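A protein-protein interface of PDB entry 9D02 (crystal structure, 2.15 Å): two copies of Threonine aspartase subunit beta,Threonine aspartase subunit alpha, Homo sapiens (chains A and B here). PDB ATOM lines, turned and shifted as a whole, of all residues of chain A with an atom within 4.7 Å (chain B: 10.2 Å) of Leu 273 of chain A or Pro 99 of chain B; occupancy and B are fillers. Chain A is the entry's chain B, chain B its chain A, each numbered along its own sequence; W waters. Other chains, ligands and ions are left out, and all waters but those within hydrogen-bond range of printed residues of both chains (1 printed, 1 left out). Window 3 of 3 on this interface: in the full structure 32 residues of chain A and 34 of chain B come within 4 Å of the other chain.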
ATOM      1  N   ALA A  43      -0.097  16.468  30.687  1.00  0.00           N
ATOM      2  CA  ALA A  43      -0.606  17.727  31.217  1.00  0.00           C
ATOM      3  C   ALA A  43      -1.857  18.106  30.439  1.00  0.00           C
ATOM      4  O   ALA A  43      -1.857  18.050  29.203  1.00  0.00           O
ATOM      5  CB  ALA A  43       0.448  18.841  31.147  1.00  0.00           C
ATOM      6  N   GLU A  44      -2.913  18.488  31.162  1.00  0.00           N
ATOM      7  CA  GLU A  44      -4.219  18.739  30.552  1.00  0.00           C
ATOM      8  C   GLU A  44      -4.967  19.772  31.391  1.00  0.00           C
ATOM      9  O   GLU A  44      -5.312  19.500  32.544  1.00  0.00           O
ATOM     10  CB  GLU A  44      -5.000  17.426  30.438  1.00  0.00           C
ATOM     11  CG  GLU A  44      -6.397  17.555  29.831  1.00  0.00           C
ATOM     12  CD  GLU A  44      -7.003  16.203  29.435  1.00  0.00           C
ATOM     13  OE1 GLU A  44      -6.362  15.138  29.661  1.00  0.00           O
ATOM     14  OE2 GLU A  44      -8.132  16.211  28.905  1.00  0.00           O
ATOM     15  N   ASN A  45      -5.203  20.961  30.837  1.00  0.00           N
ATOM     16  CA  ASN A  45      -5.963  21.968  31.569  1.00  0.00           C
ATOM     17  C   ASN A  45      -7.395  21.494  31.778  1.00  0.00           C
ATOM     18  O   ASN A  45      -7.891  20.599  31.086  1.00  0.00           O
ATOM     19  CB  ASN A  45      -5.972  23.310  30.830  1.00  0.00           C
ATOM     20  CG  ASN A  45      -4.730  24.140  31.126  1.00  0.00           C
ATOM     21  OD1 ASN A  45      -3.779  23.651  31.741  1.00  0.00           O
ATOM     22  ND2 ASN A  45      -4.726  25.386  30.675  1.00  0.00           N
ATOM     23  N   MET A 268       4.748  18.110  27.881  1.00  0.00           N
ATOM     24  CA  MET A 268       3.381  18.348  27.426  1.00  0.00           C
ATOM     25  C   MET A 268       2.859  19.652  28.031  1.00  0.00           C
ATOM     26  O   MET A 268       3.170  19.973  29.182  1.00  0.00           O
ATOM     27  CB  MET A 268       2.478  17.166  27.800  1.00  0.00           C
ATOM     28  CG  MET A 268       1.099  17.169  27.123  1.00  0.00           C
ATOM     29  SD  MET A 268       0.295  15.579  27.294  1.00  0.00           S
ATOM     30  CE  MET A 268      -1.310  15.889  26.534  1.00  0.00           C
ATOM     31  N   ASP A 269       2.095  20.417  27.241  1.00  0.00           N
ATOM     32  CA  ASP A 269       1.522  21.695  27.668  1.00  0.00           C
ATOM     33  C   ASP A 269       0.027  21.511  27.931  1.00  0.00           C
ATOM     34  O   ASP A 269      -0.709  21.085  27.040  1.00  0.00           O
ATOM     35  CB  ASP A 269       1.729  22.768  26.597  1.00  0.00           C
ATOM     36  CG  ASP A 269       1.117  24.114  26.986  1.00  0.00           C
ATOM     37  OD1 ASP A 269       1.388  24.601  28.098  1.00  0.00           O
ATOM     38  OD2 ASP A 269       0.368  24.690  26.177  1.00  0.00           O
ATOM     39  N   GLY A 270      -0.426  21.849  29.136  1.00  0.00           N
ATOM     40  CA  GLY A 270      -1.818  21.617  29.454  1.00  0.00           C
ATOM     41  C   GLY A 270      -2.758  22.514  28.674  1.00  0.00           C
ATOM     42  O   GLY A 270      -3.888  22.123  28.373  1.00  0.00           O
ATOM     43  N   LYS A 271      -2.318  23.728  28.343  1.00  0.00           N
ATOM     44  CA  LYS A 271      -3.232  24.676  27.711  1.00  0.00           C
ATOM     45  C   LYS A 271      -3.500  24.295  26.265  1.00  0.00           C
ATOM     46  O   LYS A 271      -4.654  24.165  25.855  1.00  0.00           O
ATOM     47  CB  LYS A 271      -2.676  26.091  27.789  1.00  0.00           C
ATOM     48  CG  LYS A 271      -3.608  27.139  27.171  1.00  0.00           C
ATOM     49  CD  LYS A 271      -2.986  28.530  27.225  1.00  0.00           C
ATOM     50  CE  LYS A 271      -3.890  29.588  26.591  1.00  0.00           C
ATOM     51  NZ  LYS A 271      -5.177  29.719  27.329  1.00  0.00           N
ATOM     52  N   SER A 272      -2.443  24.106  25.479  1.00  0.00           N
ATOM     53  CA  SER A 272      -2.577  23.747  24.075  1.00  0.00           C
ATOM     54  C   SER A 272      -2.694  22.249  23.849  1.00  0.00           C
ATOM     55  O   SER A 272      -3.104  21.837  22.761  1.00  0.00           O
ATOM     56  CB  SER A 272      -1.367  24.247  23.288  1.00  0.00           C
ATOM     57  OG  SER A 272      -0.235  23.470  23.660  1.00  0.00           O
ATOM     58  N   LEU A 273      -2.331  21.430  24.835  1.00  0.00           N
ATOM     59  CA  LEU A 273      -2.241  19.978  24.712  1.00  0.00           C
ATOM     60  C   LEU A 273      -1.187  19.537  23.705  1.00  0.00           C
ATOM     61  O   LEU A 273      -1.164  18.363  23.308  1.00  0.00           O
ATOM     62  CB  LEU A 273      -3.595  19.357  24.360  1.00  0.00           C
ATOM     63  CG  LEU A 273      -4.696  19.707  25.372  1.00  0.00           C
ATOM     64  CD1 LEU A 273      -6.073  19.257  24.881  1.00  0.00           C
ATOM     65  CD2 LEU A 273      -4.360  19.052  26.705  1.00  0.00           C
ATOM     66  N   ASN A 274      -0.311  20.437  23.276  1.00  0.00           N
ATOM     67  CA  ASN A 274       0.764  20.000  22.392  1.00  0.00           C
ATOM     68  C   ASN A 274       1.852  19.299  23.187  1.00  0.00           C
ATOM     69  O   ASN A 274       1.905  19.375  24.417  1.00  0.00           O
ATOM     70  CB  ASN A 274       1.344  21.168  21.605  1.00  0.00           C
ATOM     71  CG  ASN A 274       0.414  21.615  20.476  1.00  0.00           C
ATOM     72  OD1 ASN A 274      -0.325  20.802  19.909  1.00  0.00           O
ATOM     73  ND2 ASN A 274       0.426  22.903  20.168  1.00  0.00           N
ATOM     74  N   PHE A 275       2.730  18.619  22.453  1.00  0.00           N
ATOM     75  CA  PHE A 275       3.649  17.634  22.996  1.00  0.00           C
ATOM     76  C   PHE A 275       4.928  17.652  22.163  1.00  0.00           C
ATOM     77  O   PHE A 275       4.878  17.882  20.951  1.00  0.00           O
ATOM     78  CB  PHE A 275       2.966  16.264  22.965  1.00  0.00           C
ATOM     79  CG  PHE A 275       3.839  15.115  23.378  1.00  0.00           C
ATOM     80  CD1 PHE A 275       4.018  14.823  24.719  1.00  0.00           C
ATOM     81  CD2 PHE A 275       4.416  14.282  22.423  1.00  0.00           C
ATOM     82  CE1 PHE A 275       4.794  13.745  25.111  1.00  0.00           C
ATOM     83  CE2 PHE A 275       5.191  13.198  22.802  1.00  0.00           C
ATOM     84  CZ  PHE A 275       5.384  12.932  24.141  1.00  0.00           C
ATOM     85  N   GLU B  63      -0.106  13.126  13.051  1.00  0.00           N
ATOM     86  CA  GLU B  63      -0.144  13.137  14.501  1.00  0.00           C
ATOM     87  C   GLU B  63      -1.551  13.008  15.070  1.00  0.00           C
ATOM     88  O   GLU B  63      -1.682  12.809  16.282  1.00  0.00           O
ATOM     89  CB  GLU B  63       0.487  14.430  15.034  1.00  0.00           C
ATOM     90  CG  GLU B  63       1.918  14.736  14.564  1.00  0.00           C
ATOM     91  CD  GLU B  63       2.951  13.707  15.012  1.00  0.00           C
ATOM     92  OE1 GLU B  63       2.684  12.971  15.986  1.00  0.00           O
ATOM     93  OE2 GLU B  63       4.044  13.661  14.402  1.00  0.00           O
ATOM     94  N   HIS B  64      -2.592  13.031  14.228  1.00  0.00           N
ATOM     95  CA  HIS B  64      -3.961  12.920  14.730  1.00  0.00           C
ATOM     96  C   HIS B  64      -4.165  11.626  15.511  1.00  0.00           C
ATOM     97  O   HIS B  64      -4.813  11.613  16.568  1.00  0.00           O
ATOM     98  CB  HIS B  64      -4.967  12.957  13.563  1.00  0.00           C
ATOM     99  CG  HIS B  64      -4.843  14.144  12.654  1.00  0.00           C
ATOM    100  ND1 HIS B  64      -5.481  14.209  11.433  1.00  0.00           N
ATOM    101  CD2 HIS B  64      -4.180  15.317  12.792  1.00  0.00           C
ATOM    102  CE1 HIS B  64      -5.212  15.366  10.855  1.00  0.00           C
ATOM    103  NE2 HIS B  64      -4.427  16.058  11.661  1.00  0.00           N
ATOM    104  N   VAL B  66      -1.856   9.747  16.975  1.00  0.00           N
ATOM    105  CA  VAL B  66      -1.073   9.749  18.207  1.00  0.00           C
ATOM    106  C   VAL B  66      -1.801  10.516  19.310  1.00  0.00           C
ATOM    107  O   VAL B  66      -2.033   9.982  20.398  1.00  0.00           O
ATOM    108  CB  VAL B  66       0.329  10.324  17.948  1.00  0.00           C
ATOM    109  CG1 VAL B  66       1.183  10.359  19.255  1.00  0.00           C
ATOM    110  CG2 VAL B  66       1.025   9.521  16.849  1.00  0.00           C
ATOM    111  N   ARG B  67      -2.172  11.777  19.043  1.00  0.00           N
ATOM    112  CA  ARG B  67      -2.659  12.652  20.104  1.00  0.00           C
ATOM    113  C   ARG B  67      -3.898  12.079  20.785  1.00  0.00           C
ATOM    114  O   ARG B  67      -4.112  12.318  21.977  1.00  0.00           O
ATOM    115  CB  ARG B  67      -2.963  14.058  19.562  1.00  0.00           C
ATOM    116  CG  ARG B  67      -1.770  14.766  18.900  1.00  0.00           C
ATOM    117  CD  ARG B  67      -0.461  14.534  19.652  1.00  0.00           C
ATOM    118  NE  ARG B  67       0.665  15.252  19.055  1.00  0.00           N
ATOM    119  CZ  ARG B  67       0.894  16.556  19.188  1.00  0.00           C
ATOM    120  NH1 ARG B  67       1.950  17.099  18.597  1.00  0.00           N
ATOM    121  NH2 ARG B  67       0.082  17.319  19.909  1.00  0.00           N
ATOM    122  N   THR B  68      -4.692  11.290  20.075  1.00  0.00           N
ATOM    123  CA  THR B  68      -5.904  10.722  20.649  1.00  0.00           C
ATOM    124  C   THR B  68      -5.730   9.277  21.114  1.00  0.00           C
ATOM    125  O   THR B  68      -6.692   8.683  21.604  1.00  0.00           O
ATOM    126  CB  THR B  68      -7.054  10.795  19.629  1.00  0.00           C
ATOM    127  OG1 THR B  68      -6.691  10.070  18.442  1.00  0.00           O
ATOM    128  CG2 THR B  68      -7.377  12.257  19.261  1.00  0.00           C
ATOM    129  N   THR B  90     -16.822   6.877  19.166  1.00  0.00           N
ATOM    130  CA  THR B  90     -15.406   7.133  19.384  1.00  0.00           C
ATOM    131  C   THR B  90     -14.831   7.961  18.247  1.00  0.00           C
ATOM    132  O   THR B  90     -14.131   8.956  18.478  1.00  0.00           O
ATOM    133  CB  THR B  90     -14.654   5.813  19.511  1.00  0.00           C
ATOM    134  OG1 THR B  90     -15.269   5.030  20.532  1.00  0.00           O
ATOM    135  CG2 THR B  90     -13.176   6.066  19.862  1.00  0.00           C
ATOM    136  N   MET B  91     -15.159   7.585  17.005  1.00  0.00           N
ATOM    137  CA  MET B  91     -14.651   8.309  15.842  1.00  0.00           C
ATOM    138  C   MET B  91     -15.140   9.746  15.824  1.00  0.00           C
ATOM    139  O   MET B  91     -14.379  10.666  15.486  1.00  0.00           O
ATOM    140  CB  MET B  91     -15.060   7.594  14.554  1.00  0.00           C
ATOM    141  CG  MET B  91     -14.406   6.226  14.397  1.00  0.00           C
ATOM    142  SD  MET B  91     -12.613   6.338  14.154  1.00  0.00           S
ATOM    143  CE  MET B  91     -12.542   7.071  12.523  1.00  0.00           C
ATOM    144  N   GLN B  92     -16.398   9.964  16.215  1.00  0.00           N
ATOM    145  CA  GLN B  92     -16.953  11.308  16.199  1.00  0.00           C
ATOM    146  C   GLN B  92     -16.429  12.142  17.362  1.00  0.00           C
ATOM    147  O   GLN B  92     -16.068  13.306  17.180  1.00  0.00           O
ATOM    148  CB  GLN B  92     -18.490  11.239  16.242  1.00  0.00           C
ATOM    149  CG  GLN B  92     -19.123  10.785  14.928  1.00  0.00           C
ATOM    150  CD  GLN B  92     -20.634  10.494  15.043  1.00  0.00           C
ATOM    151  OE1 GLN B  92     -21.143  10.158  16.118  1.00  0.00           O
ATOM    152  NE2 GLN B  92     -21.343  10.633  13.933  1.00  0.00           N
ATOM    153  N   ASN B  93     -16.420  11.576  18.569  1.00  0.00           N
ATOM    154  CA  ASN B  93     -16.202  12.352  19.786  1.00  0.00           C
ATOM    155  C   ASN B  93     -14.732  12.374  20.190  1.00  0.00           C
ATOM    156  O   ASN B  93     -14.214  13.422  20.574  1.00  0.00           O
ATOM    157  CB  ASN B  93     -17.036  11.788  20.943  1.00  0.00           C
ATOM    158  CG  ASN B  93     -18.539  11.799  20.662  1.00  0.00           C
ATOM    159  OD1 ASN B  93     -19.053  12.656  19.944  1.00  0.00           O
ATOM    160  ND2 ASN B  93     -19.243  10.827  21.227  1.00  0.00           N
ATOM    161  N   LYS B  94     -14.058  11.227  20.142  1.00  0.00           N
ATOM    162  CA  LYS B  94     -12.673  11.150  20.595  1.00  0.00           C
ATOM    163  C   LYS B  94     -11.674  11.298  19.463  1.00  0.00           C
ATOM    164  O   LYS B  94     -10.478  11.433  19.730  1.00  0.00           O
ATOM    165  CB  LYS B  94     -12.410   9.813  21.316  1.00  0.00           C
ATOM    166  CG  LYS B  94     -13.390   9.515  22.463  1.00  0.00           C
ATOM    167  CD  LYS B  94     -13.190  10.460  23.623  1.00  0.00           C
ATOM    168  CE  LYS B  94     -13.678   9.829  24.917  1.00  0.00           C
ATOM    169  NZ  LYS B  94     -13.110   8.452  25.030  1.00  0.00           N
ATOM    170  N   PHE B  95     -12.127  11.311  18.215  1.00  0.00           N
ATOM    171  CA  PHE B  95     -11.234  11.520  17.088  1.00  0.00           C
ATOM    172  C   PHE B  95     -11.553  12.861  16.437  1.00  0.00           C
ATOM    173  O   PHE B  95     -10.861  13.844  16.696  1.00  0.00           O
ATOM    174  CB  PHE B  95     -11.333  10.344  16.106  1.00  0.00           C
ATOM    175  CG  PHE B  95     -10.245  10.323  15.055  1.00  0.00           C
ATOM    176  CD1 PHE B  95      -8.906  10.408  15.414  1.00  0.00           C
ATOM    177  CD2 PHE B  95     -10.566  10.181  13.706  1.00  0.00           C
ATOM    178  CE1 PHE B  95      -7.895  10.377  14.444  1.00  0.00           C
ATOM    179  CE2 PHE B  95      -9.572  10.148  12.730  1.00  0.00           C
ATOM    180  CZ  PHE B  95      -8.226  10.251  13.099  1.00  0.00           C
ATOM    181  N   ILE B  96     -12.657  12.962  15.697  1.00  0.00           N
ATOM    182  CA  ILE B  96     -12.956  14.184  14.956  1.00  0.00           C
ATOM    183  C   ILE B  96     -13.069  15.379  15.887  1.00  0.00           C
ATOM    184  O   ILE B  96     -12.568  16.467  15.581  1.00  0.00           O
ATOM    185  CB  ILE B  96     -14.245  13.996  14.138  1.00  0.00           C
ATOM    186  CG1 ILE B  96     -13.952  13.192  12.875  1.00  0.00           C
ATOM    187  CG2 ILE B  96     -14.871  15.357  13.810  1.00  0.00           C
ATOM    188  CD1 ILE B  96     -15.126  13.138  11.934  1.00  0.00           C
ATOM    189  N   SER B  97     -13.756  15.220  17.016  1.00  0.00           N
ATOM    190  CA  SER B  97     -14.008  16.352  17.904  1.00  0.00           C
ATOM    191  C   SER B  97     -13.097  16.355  19.117  1.00  0.00           C
ATOM    192  O   SER B  97     -13.403  17.012  20.112  1.00  0.00           O
ATOM    193  CB  SER B  97     -15.473  16.388  18.339  1.00  0.00           C
ATOM    194  OG  SER B  97     -16.274  16.588  17.201  1.00  0.00           O
ATOM    195  N   SER B  98     -11.993  15.633  19.070  1.00  0.00           N
ATOM    196  CA  SER B  98     -11.092  15.676  20.204  1.00  0.00           C
ATOM    197  C   SER B  98     -10.639  17.113  20.441  1.00  0.00           C
ATOM    198  O   SER B  98     -10.403  17.854  19.482  1.00  0.00           O
ATOM    199  CB  SER B  98      -9.871  14.791  19.966  1.00  0.00           C
ATOM    200  OG  SER B  98      -8.894  15.105  20.932  1.00  0.00           O
ATOM    201  N   PRO B  99     -10.503  17.541  21.699  1.00  0.00           N
ATOM    202  CA  PRO B  99      -9.828  18.820  21.964  1.00  0.00           C
ATOM    203  C   PRO B  99      -8.341  18.782  21.631  1.00  0.00           C
ATOM    204  O   PRO B  99      -7.724  19.847  21.477  1.00  0.00           O
ATOM    205  CB  PRO B  99     -10.069  19.035  23.462  1.00  0.00           C
ATOM    206  CG  PRO B  99     -10.140  17.647  24.001  1.00  0.00           C
ATOM    207  CD  PRO B  99     -10.876  16.855  22.948  1.00  0.00           C
ATOM    208  N   PHE B 100      -7.747  17.589  21.541  1.00  0.00           N
ATOM    209  CA  PHE B 100      -6.337  17.443  21.199  1.00  0.00           C
ATOM    210  C   PHE B 100      -6.057  17.795  19.751  1.00  0.00           C
ATOM    211  O   PHE B 100      -4.888  17.862  19.362  1.00  0.00           O
ATOM    212  CB  PHE B 100      -5.869  16.005  21.477  1.00  0.00           C
ATOM    213  CG  PHE B 100      -5.903  15.642  22.923  1.00  0.00           C
ATOM    214  CD1 PHE B 100      -4.766  15.769  23.706  1.00  0.00           C
ATOM    215  CD2 PHE B 100      -7.082  15.222  23.517  1.00  0.00           C
ATOM    216  CE1 PHE B 100      -4.801  15.464  25.053  1.00  0.00           C
ATOM    217  CE2 PHE B 100      -7.132  14.917  24.867  1.00  0.00           C
ATOM    218  CZ  PHE B 100      -5.993  15.036  25.638  1.00  0.00           C
ATOM    219  N   LEU B 101      -7.097  18.005  18.949  1.00  0.00           N
ATOM    220  CA  LEU B 101      -6.961  18.334  17.539  1.00  0.00           C
ATOM    221  C   LEU B 101      -7.790  19.570  17.218  1.00  0.00           C
ATOM    222  O   LEU B 101      -8.299  19.717  16.102  1.00  0.00           O
ATOM    223  CB  LEU B 101      -7.374  17.147  16.662  1.00  0.00           C
ATOM    224  CG  LEU B 101      -6.739  15.782  16.954  1.00  0.00           C
ATOM    225  CD1 LEU B 101      -7.602  14.650  16.426  1.00  0.00           C
ATOM    226  CD2 LEU B 101      -5.369  15.711  16.332  1.00  0.00           C
ATOM    227  N   ALA B 102      -7.926  20.466  18.199  1.00  0.00           N
ATOM    228  CA  ALA B 102      -8.900  21.551  18.102  1.00  0.00           C
ATOM    229  C   ALA B 102      -8.518  22.547  17.016  1.00  0.00           C
ATOM    230  O   ALA B 102      -9.326  22.859  16.135  1.00  0.00           O
ATOM    231  CB  ALA B 102      -9.038  22.250  19.455  1.00  0.00           C
ATOM    232  N   SER B 103      -7.287  23.057  17.060  1.00  0.00           N
ATOM    233  CA  SER B 103      -6.831  23.990  16.038  1.00  0.00           C
ATOM    234  C   SER B 103      -6.584  23.317  14.696  1.00  0.00           C
ATOM    235  O   SER B 103      -6.189  23.999  13.744  1.00  0.00           O
ATOM    236  CB  SER B 103      -5.560  24.695  16.509  1.00  0.00           C
ATOM    237  OG  SER B 103      -4.598  23.737  16.903  1.00  0.00           O
ATOM    238  N   GLU B 104      -6.800  22.008  14.597  1.00  0.00           N
ATOM    239  CA  GLU B 104      -6.613  21.299  13.343  1.00  0.00           C
ATOM    240  C   GLU B 104      -7.872  21.406  12.499  1.00  0.00           C
ATOM    241  O   GLU B 104      -8.983  21.187  12.991  1.00  0.00           O
ATOM    242  CB  GLU B 104      -6.261  19.836  13.603  1.00  0.00           C
ATOM    243  CG  GLU B 104      -4.864  19.675  14.181  1.00  0.00           C
ATOM    244  CD  GLU B 104      -3.834  20.411  13.351  1.00  0.00           C
ATOM    245  OE1 GLU B 104      -3.761  20.133  12.135  1.00  0.00           O
ATOM    246  OE2 GLU B 104      -3.120  21.284  13.901  1.00  0.00           O
ATOM    247  N   VAL B 107      -9.638  16.127  10.366  1.00  0.00           N
ATOM    248  CA  VAL B 107      -8.964  15.027  11.051  1.00  0.00           C
ATOM    249  C   VAL B 107      -9.087  13.795  10.162  1.00  0.00           C
ATOM    250  O   VAL B 107     -10.199  13.300   9.927  1.00  0.00           O
ATOM    251  CB  VAL B 107      -9.573  14.760  12.440  1.00  0.00           C
ATOM    252  CG1 VAL B 107      -8.927  13.573  13.073  1.00  0.00           C
ATOM    253  CG2 VAL B 107      -9.445  15.990  13.337  1.00  0.00           C
HETATM  254  O   HOH W   1      -1.269  16.080  22.143  1.00  0.00           O
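The side-chain hydroxyl (OG) of Ser 98 of chain B sits at hydrogen-bond distance from the backbone NH (N) of Phe 100 of chain B, 2.8 Å away.
The backbone NH (N) of Ala 43 of chain A sits at hydrogen-bond distance from the side-chain sulfur (SD) of Met 268 of chain A, at 3.5 Å.
The backbone carbonyl oxygen (O) of Asn 274 of chain A sits at hydrogen-bond distance from the backbone NH (N) of Asp 269 of chain A, at 3.0 Å.
The side-chain hydroxyl (OG) of Ser 272 of chain A lies close to the backbone NH (N) of Asn 274 of chain A, 3.1 Å away.
Of the 21 printed residues of chain B, 3 touch a printed residue of chain A.
Printed residues of chain B that touch a printed residue of chain A: Arg 67, Pro 99 and Phe 100.
Hydrophobic or aromatic side chains of chain B within 4 Å of the printed part of chain A: Phe 100.
Along chain B the printed residues that touch a printed residue of chain A span positions 67 to 100.
Among the printed residues, 6 pairs touch across the chains.
Among the printed residues, no Asp or Glu carboxylate lies within 4 Å of a Lys or Arg side-chain nitrogen of the other chain.
No residue of chain B comes within 4 Å of Glu 44 of chain A.
Of the printed residues of chain B, Met 268 of chain A touches Phe 100 (3.8 Å).
No residue of chain B comes within 4 Å of Asp 269 of chain A.
No residue of chain B comes within 4 Å of Ser 272 of chain A.
Of chain B, only Arg 67 (3.8 Å), Pro 99 (3.8 Å) and Phe 100 (3.8 Å) come within 4 Å of Leu 273 of chain A.
Asn 274 of chain A touches just one residue of chain B: Arg 67.
Printed residues of chain B within 4 Å of Phe 275 of chain A: Arg 67 (3.8 Å).
Pro 99 of chain B touches one residue of chain A.
The nearest printed residue of chain A that does not touch Pro 99 of chain B is Ser 272 of chain A (5.2 Å).
The nearest printed residue of chain A that does not touch Phe 100 of chain B is Glu 44 of chain A (4.04 Å).
Among the printed residues, pairs that only touch across the chains: Asn 274 of chain A with Arg 67 of chain B (3.5 Å), Leu 273 of chain A with Arg 67 of chain B (3.8 Å), Met 268 of chain A with Phe 100 of chain B (3.8 Å), Leu 273 of chain A with Pro 99 of chain B (3.8 Å), Leu 273 of chain A with Phe 100 of chain B (3.8 Å) and Phe 275 of chain A with Arg 67 of chain B (3.8 Å).
No position is printed for both chains.
Of the 6 pairs that touch across the chains among the printed residues, none has its exchanged pair printed and touching as well.
Water W1 bridges O of Leu 273 of chain A and NH2 of Arg 67 of chain B.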
